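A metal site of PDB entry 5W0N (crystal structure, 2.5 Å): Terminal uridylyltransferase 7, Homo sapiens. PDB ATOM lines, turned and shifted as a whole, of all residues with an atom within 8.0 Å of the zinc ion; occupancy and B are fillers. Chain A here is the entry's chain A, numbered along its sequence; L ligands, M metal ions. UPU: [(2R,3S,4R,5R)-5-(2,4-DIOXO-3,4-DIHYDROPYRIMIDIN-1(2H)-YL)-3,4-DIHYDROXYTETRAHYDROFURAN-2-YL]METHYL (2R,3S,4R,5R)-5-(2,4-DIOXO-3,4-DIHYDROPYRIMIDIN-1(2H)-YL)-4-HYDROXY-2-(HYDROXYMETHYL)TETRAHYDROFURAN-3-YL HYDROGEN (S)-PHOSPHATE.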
ATOM      1  N   CYS A 384     -26.563   0.148   3.466  1.00  0.00           N
ATOM      2  CA  CYS A 384     -26.151  -0.630   4.625  1.00  0.00           C
ATOM      3  C   CYS A 384     -27.286  -0.767   5.633  1.00  0.00           C
ATOM      4  O   CYS A 384     -28.149   0.105   5.771  1.00  0.00           O
ATOM      5  CB  CYS A 384     -24.951   0.015   5.312  1.00  0.00           C
ATOM      6  SG  CYS A 384     -23.470   0.065   4.281  1.00  0.00           S
ATOM      7  N   CYS A 385     -27.270  -1.889   6.347  1.00  0.00           N
ATOM      8  CA  CYS A 385     -28.171  -2.118   7.463  1.00  0.00           C
ATOM      9  C   CYS A 385     -27.984  -1.029   8.522  1.00  0.00           C
ATOM     10  O   CYS A 385     -26.855  -0.621   8.818  1.00  0.00           O
ATOM     11  CB  CYS A 385     -27.916  -3.504   8.063  1.00  0.00           C
ATOM     12  SG  CYS A 385     -28.780  -3.869   9.606  1.00  0.00           S
ATOM     13  N   ARG A 386     -29.092  -0.550   9.077  1.00  0.00           N
ATOM     14  CA  ARG A 386     -29.030   0.510  10.072  1.00  0.00           C
ATOM     15  C   ARG A 386     -28.585   0.023  11.442  1.00  0.00           C
ATOM     16  O   ARG A 386     -28.347   0.849  12.325  1.00  0.00           O
ATOM     17  CB  ARG A 386     -30.399   1.195  10.187  1.00  0.00           C
ATOM     18  CG  ARG A 386     -31.489   0.303  10.775  1.00  0.00           C
ATOM     19  CD  ARG A 386     -32.839   1.007  10.771  1.00  0.00           C
ATOM     20  NE  ARG A 386     -33.303   1.282   9.412  1.00  0.00           N
ATOM     21  CZ  ARG A 386     -34.450   1.891   9.122  1.00  0.00           C
ATOM     22  NH1 ARG A 386     -35.259   2.307  10.097  1.00  0.00           N
ATOM     23  NH2 ARG A 386     -34.782   2.096   7.853  1.00  0.00           N
ATOM     24  N   ILE A 387     -28.463  -1.286  11.635  1.00  0.00           N
ATOM     25  CA  ILE A 387     -28.046  -1.824  12.924  1.00  0.00           C
ATOM     26  C   ILE A 387     -26.536  -2.015  12.989  1.00  0.00           C
ATOM     27  O   ILE A 387     -25.882  -1.561  13.933  1.00  0.00           O
ATOM     28  CB  ILE A 387     -28.794  -3.143  13.205  1.00  0.00           C
ATOM     29  CG1 ILE A 387     -30.307  -2.905  13.202  1.00  0.00           C
ATOM     30  CG2 ILE A 387     -28.343  -3.748  14.523  1.00  0.00           C
ATOM     31  CD1 ILE A 387     -31.139  -4.172  13.302  1.00  0.00           C
ATOM     32  N   CYS A 388     -25.960  -2.686  11.990  1.00  0.00           N
ATOM     33  CA  CYS A 388     -24.547  -3.013  11.993  1.00  0.00           C
ATOM     34  C   CYS A 388     -23.736  -2.246  10.951  1.00  0.00           C
ATOM     35  O   CYS A 388     -22.517  -2.122  11.121  1.00  0.00           O
ATOM     36  CB  CYS A 388     -24.340  -4.518  11.755  1.00  0.00           C
ATOM     37  SG  CYS A 388     -24.851  -5.073  10.113  1.00  0.00           S
ATOM     38  N   GLY A 389     -24.372  -1.735   9.899  1.00  0.00           N
ATOM     39  CA  GLY A 389     -23.667  -1.009   8.869  1.00  0.00           C
ATOM     40  C   GLY A 389     -23.139  -1.863   7.732  1.00  0.00           C
ATOM     41  O   GLY A 389     -22.352  -1.357   6.925  1.00  0.00           O
ATOM     42  N   LYS A 390     -23.554  -3.117   7.645  1.00  0.00           N
ATOM     43  CA  LYS A 390     -23.150  -4.016   6.573  1.00  0.00           C
ATOM     44  C   LYS A 390     -24.256  -4.125   5.532  1.00  0.00           C
ATOM     45  O   LYS A 390     -25.433  -3.880   5.824  1.00  0.00           O
ATOM     46  CB  LYS A 390     -22.801  -5.406   7.117  1.00  0.00           C
ATOM     47  CG  LYS A 390     -21.671  -5.434   8.138  1.00  0.00           C
ATOM     48  CD  LYS A 390     -20.357  -4.948   7.537  1.00  0.00           C
ATOM     49  CE  LYS A 390     -19.168  -5.303   8.421  1.00  0.00           C
ATOM     50  NZ  LYS A 390     -18.885  -6.759   8.417  1.00  0.00           N
ATOM     51  N   ILE A 391     -23.870  -4.513   4.327  1.00  0.00           N
ATOM     52  CA  ILE A 391     -24.812  -4.714   3.245  1.00  0.00           C
ATOM     53  C   ILE A 391     -25.153  -6.196   3.156  1.00  0.00           C
ATOM     54  O   ILE A 391     -24.457  -7.058   3.692  1.00  0.00           O
ATOM     55  CB  ILE A 391     -24.254  -4.194   1.895  1.00  0.00           C
ATOM     56  CG1 ILE A 391     -22.992  -4.959   1.492  1.00  0.00           C
ATOM     57  CG2 ILE A 391     -23.968  -2.695   1.974  1.00  0.00           C
ATOM     58  CD1 ILE A 391     -23.238  -6.087   0.510  1.00  0.00           C
ATOM     59  N   GLY A 392     -26.262  -6.496   2.473  1.00  0.00           N
ATOM     60  CA  GLY A 392     -26.585  -7.856   2.110  1.00  0.00           C
ATOM     61  C   GLY A 392     -27.523  -8.613   3.029  1.00  0.00           C
ATOM     62  O   GLY A 392     -27.546  -9.847   2.973  1.00  0.00           O
ATOM     63  N   HIS A 393     -28.291  -7.931   3.872  1.00  0.00           N
ATOM     64  CA  HIS A 393     -29.230  -8.630   4.732  1.00  0.00           C
ATOM     65  C   HIS A 393     -30.298  -7.662   5.234  1.00  0.00           C
ATOM     66  O   HIS A 393     -30.047  -6.471   5.410  1.00  0.00           O
ATOM     67  CB  HIS A 393     -28.527  -9.296   5.930  1.00  0.00           C
ATOM     68  CG  HIS A 393     -27.998  -8.324   6.944  1.00  0.00           C
ATOM     69  ND1 HIS A 393     -26.662  -8.078   7.108  1.00  0.00           N
ATOM     70  CD2 HIS A 393     -28.643  -7.549   7.848  1.00  0.00           C
ATOM     71  CE1 HIS A 393     -26.486  -7.187   8.071  1.00  0.00           C
ATOM     72  NE2 HIS A 393     -27.671  -6.852   8.538  1.00  0.00           N
ATOM     73  N   PHE A 394     -31.490  -8.200   5.463  1.00  0.00           N
ATOM     74  CA  PHE A 394     -32.563  -7.433   6.072  1.00  0.00           C
ATOM     75  C   PHE A 394     -32.415  -7.424   7.583  1.00  0.00           C
ATOM     76  O   PHE A 394     -31.707  -8.240   8.176  1.00  0.00           O
ATOM     77  CB  PHE A 394     -33.926  -7.988   5.654  1.00  0.00           C
ATOM     78  CG  PHE A 394     -34.221  -7.836   4.191  1.00  0.00           C
ATOM     79  CD1 PHE A 394     -34.465  -6.585   3.642  1.00  0.00           C
ATOM     80  CD2 PHE A 394     -34.245  -8.944   3.355  1.00  0.00           C
ATOM     81  CE1 PHE A 394     -34.727  -6.440   2.293  1.00  0.00           C
ATOM     82  CE2 PHE A 394     -34.507  -8.800   2.006  1.00  0.00           C
ATOM     83  CZ  PHE A 394     -34.751  -7.553   1.478  1.00  0.00           C
ATOM     84  N   MET A 395     -33.107  -6.480   8.229  1.00  0.00           N
ATOM     85  CA  MET A 395     -32.891  -6.242   9.651  1.00  0.00           C
ATOM     86  C   MET A 395     -33.238  -7.459  10.500  1.00  0.00           C
ATOM     87  O   MET A 395     -32.652  -7.646  11.569  1.00  0.00           O
ATOM     88  CB  MET A 395     -33.710  -5.027  10.102  1.00  0.00           C
ATOM     89  CG  MET A 395     -32.887  -3.750  10.180  1.00  0.00           C
ATOM     90  SD  MET A 395     -33.913  -2.302  10.494  1.00  0.00           S
ATOM     91  CE  MET A 395     -34.642  -2.063   8.875  1.00  0.00           C
ATOM     92  N   LYS A 396     -34.185  -8.282  10.056  1.00  0.00           N
ATOM     93  CA  LYS A 396     -34.522  -9.490  10.806  1.00  0.00           C
ATOM     94  C   LYS A 396     -33.379 -10.498  10.806  1.00  0.00           C
ATOM     95  O   LYS A 396     -33.363 -11.397  11.664  1.00  0.00           O
ATOM     96  CB  LYS A 396     -35.782 -10.121  10.236  1.00  0.00           C
ATOM     97  CG  LYS A 396     -37.032  -9.274  10.403  1.00  0.00           C
ATOM     98  CD  LYS A 396     -38.285 -10.014   9.967  1.00  0.00           C
ATOM     99  CE  LYS A 396     -39.545  -9.210  10.284  1.00  0.00           C
ATOM    100  NZ  LYS A 396     -40.786  -9.955   9.944  1.00  0.00           N
ATOM    101  N   ASP A 397     -32.420 -10.365   9.897  1.00  0.00           N
ATOM    102  CA  ASP A 397     -31.297 -11.286   9.776  1.00  0.00           C
ATOM    103  C   ASP A 397     -29.996 -10.694  10.303  1.00  0.00           C
ATOM    104  O   ASP A 397     -28.940 -11.307  10.139  1.00  0.00           O
ATOM    105  CB  ASP A 397     -31.121 -11.709   8.320  1.00  0.00           C
ATOM    106  CG  ASP A 397     -32.439 -12.006   7.622  1.00  0.00           C
ATOM    107  OD1 ASP A 397     -33.282 -12.719   8.211  1.00  0.00           O
ATOM    108  OD2 ASP A 397     -32.643 -11.516   6.494  1.00  0.00           O
ATOM    109  N   CYS A 398     -30.058  -9.528  10.951  1.00  0.00           N
ATOM    110  CA  CYS A 398     -28.844  -8.865  11.403  1.00  0.00           C
ATOM    111  C   CYS A 398     -28.267  -9.583  12.624  1.00  0.00           C
ATOM    112  O   CYS A 398     -29.017  -9.940  13.548  1.00  0.00           O
ATOM    113  CB  CYS A 398     -29.133  -7.409  11.743  1.00  0.00           C
ATOM    114  SG  CYS A 398     -27.678  -6.428  12.162  1.00  0.00           S
ATOM    115  N   PRO A 399     -26.949  -9.819  12.672  1.00  0.00           N
ATOM    116  CA  PRO A 399     -26.379 -10.402  13.895  1.00  0.00           C
ATOM    117  C   PRO A 399     -26.464  -9.487  15.107  1.00  0.00           C
ATOM    118  O   PRO A 399     -26.719  -9.966  16.220  1.00  0.00           O
ATOM    119  CB  PRO A 399     -24.916 -10.671  13.502  1.00  0.00           C
ATOM    120  CG  PRO A 399     -24.915 -10.723  12.018  1.00  0.00           C
ATOM    121  CD  PRO A 399     -25.976  -9.759  11.574  1.00  0.00           C
ATOM    122  N   MET A 400     -26.257  -8.187  14.927  1.00  0.00           N
ATOM    123  CA  MET A 400     -26.265  -7.235  16.029  1.00  0.00           C
ATOM    124  C   MET A 400     -27.677  -6.871  16.492  1.00  0.00           C
ATOM    125  O   MET A 400     -27.832  -5.898  17.251  1.00  0.00           O
ATOM    126  CB  MET A 400     -25.521  -5.958  15.626  1.00  0.00           C
ATOM    127  CG  MET A 400     -24.035  -6.164  15.300  1.00  0.00           C
ATOM    128  SD  MET A 400     -23.032  -6.642  16.723  1.00  0.00           S
ATOM    129  CE  MET A 400     -23.004  -8.423  16.571  1.00  0.00           C
ATOM    130  N   ARG A 401     -28.701  -7.605  16.060  1.00  0.00           N
ATOM    131  CA  ARG A 401     -30.063  -7.369  16.528  1.00  0.00           C
ATOM    132  C   ARG A 401     -30.260  -7.942  17.927  1.00  0.00           C
ATOM    133  O   ARG A 401     -30.462  -7.205  18.895  1.00  0.00           O
ATOM    134  CB  ARG A 401     -31.065  -7.997  15.551  1.00  0.00           C
ATOM    135  CG  ARG A 401     -32.526  -7.879  15.971  1.00  0.00           C
ATOM    136  CD  ARG A 401     -33.439  -8.501  14.922  1.00  0.00           C
ATOM    137  NE  ARG A 401     -34.853  -8.406  15.272  1.00  0.00           N
ATOM    138  CZ  ARG A 401     -35.533  -9.325  15.953  1.00  0.00           C
ATOM    139  NH1 ARG A 401     -34.930 -10.435  16.366  1.00  0.00           N
ATOM    140  NH2 ARG A 401     -36.823  -9.140  16.220  1.00  0.00           N
HETATM  141  O2A UPU L   1     -12.379 -14.896  -0.820  1.00  0.00           O
HETATM  142  C2A UPU L   1     -13.110 -13.999  -1.191  1.00  0.00           C
HETATM  143  N3A UPU L   1     -13.293 -13.702  -2.639  1.00  0.00           N
HETATM  144  C4A UPU L   1     -14.176 -12.628  -3.063  1.00  0.00           C
HETATM  145  O4A UPU L   1     -14.318 -12.399  -4.215  1.00  0.00           O
HETATM  146  C5A UPU L   1     -14.911 -11.807  -2.047  1.00  0.00           C
HETATM  147  C6A UPU L   1     -14.732 -12.098  -0.592  1.00  0.00           C
HETATM  148  N1A UPU L   1     -13.838 -13.191  -0.173  1.00  0.00           N
HETATM  149 C1'A UPU L   1     -13.645 -13.490   1.220  1.00  0.00           C
HETATM  150 O4'A UPU L   1     -14.908 -12.938   2.054  1.00  0.00           O
HETATM  151 C2'A UPU L   1     -12.572 -12.888   1.679  1.00  0.00           C
HETATM  152 O2'A UPU L   1     -11.818 -13.803   2.571  1.00  0.00           O
HETATM  153 C3'A UPU L   1     -13.079 -11.681   2.485  1.00  0.00           C
HETATM  154 O3'A UPU L   1     -12.223 -11.397   3.513  1.00  0.00           O
HETATM  155 C4'A UPU L   1     -14.431 -12.182   3.009  1.00  0.00           C
HETATM  156 C5'A UPU L   1     -15.398 -10.967   3.219  1.00  0.00           C
HETATM  157 O5'A UPU L   1     -15.464 -10.302   1.965  1.00  0.00           O
HETATM  158  P   UPU L   1     -15.971  -8.696   1.954  1.00  0.00           P
HETATM  159  O1  UPU L   1     -15.195  -7.905   2.952  1.00  0.00           O
HETATM  160  O2  UPU L   1     -15.763  -8.152   0.594  1.00  0.00           O
HETATM  161 O3'B UPU L   1     -17.575  -8.686   2.345  1.00  0.00           O
HETATM  162 C3'B UPU L   1     -18.548  -9.535   1.553  1.00  0.00           C
HETATM  163 C4'B UPU L   1     -19.492  -8.571   0.727  1.00  0.00           C
HETATM  164 C5'B UPU L   1     -20.162  -9.234  -0.307  1.00  0.00           C
HETATM  165 O5'B UPU L   1     -19.299  -9.292  -1.463  1.00  0.00           O
HETATM  166 O4'B UPU L   1     -20.463  -8.075   1.771  1.00  0.00           O
HETATM  167 C2'B UPU L   1     -19.341 -10.076   2.310  1.00  0.00           C
HETATM  168 O2'B UPU L   1     -18.661 -10.730   3.461  1.00  0.00           O
HETATM  169 C1'B UPU L   1     -20.258  -8.787   2.820  1.00  0.00           C
HETATM  170  N1B UPU L   1     -21.519  -9.232   3.372  1.00  0.00           N
HETATM  171  C2B UPU L   1     -21.783  -9.020   4.834  1.00  0.00           C
HETATM  172  O2B UPU L   1     -20.936  -8.491   5.522  1.00  0.00           O
HETATM  173  C6B UPU L   1     -22.535  -9.869   2.522  1.00  0.00           C
HETATM  174  C5B UPU L   1     -23.831 -10.304   3.117  1.00  0.00           C
HETATM  175  C4B UPU L   1     -24.098 -10.092   4.593  1.00  0.00           C
HETATM  176  N3B UPU L   1     -23.071  -9.450   5.431  1.00  0.00           N
HETATM  177  O4B UPU L   1     -25.122 -10.446   5.082  1.00  0.00           O
HETATM  178 ZN    ZN M   1     -27.117  -5.612  10.057  1.00  0.00          ZN
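The zinc ion is bound by NE2 of His 393 (2.0 Å), SG of Cys 398 (2.3 Å), SG of Cys 388 (2.3 Å) and SG of Cys 385 (2.5 Å).
An oxygen (O4B) of the ligand is in hydrogen-bond range of a ring nitrogen (ND1) of His 393 (3.5 Å).
The backbone carbonyl oxygen of Ile 391 sits close to a nitrogen (N3B) of the ligand.
The backbone NH (N) of Met 400 lies close to the side-chain sulfur (SG) of Cys 398, at 3.6 Å.
N of Lys 390 lies close to SG of Cys 388 (3.4 Å).
SG of Cys 385 lies close to N of Ile 387, 3.3 Å away.
N of Cys 385 is in hydrogen-bond range of O of Lys 390.
Of the 18 residues printed, 4 come within 4 Å of the zinc ion.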
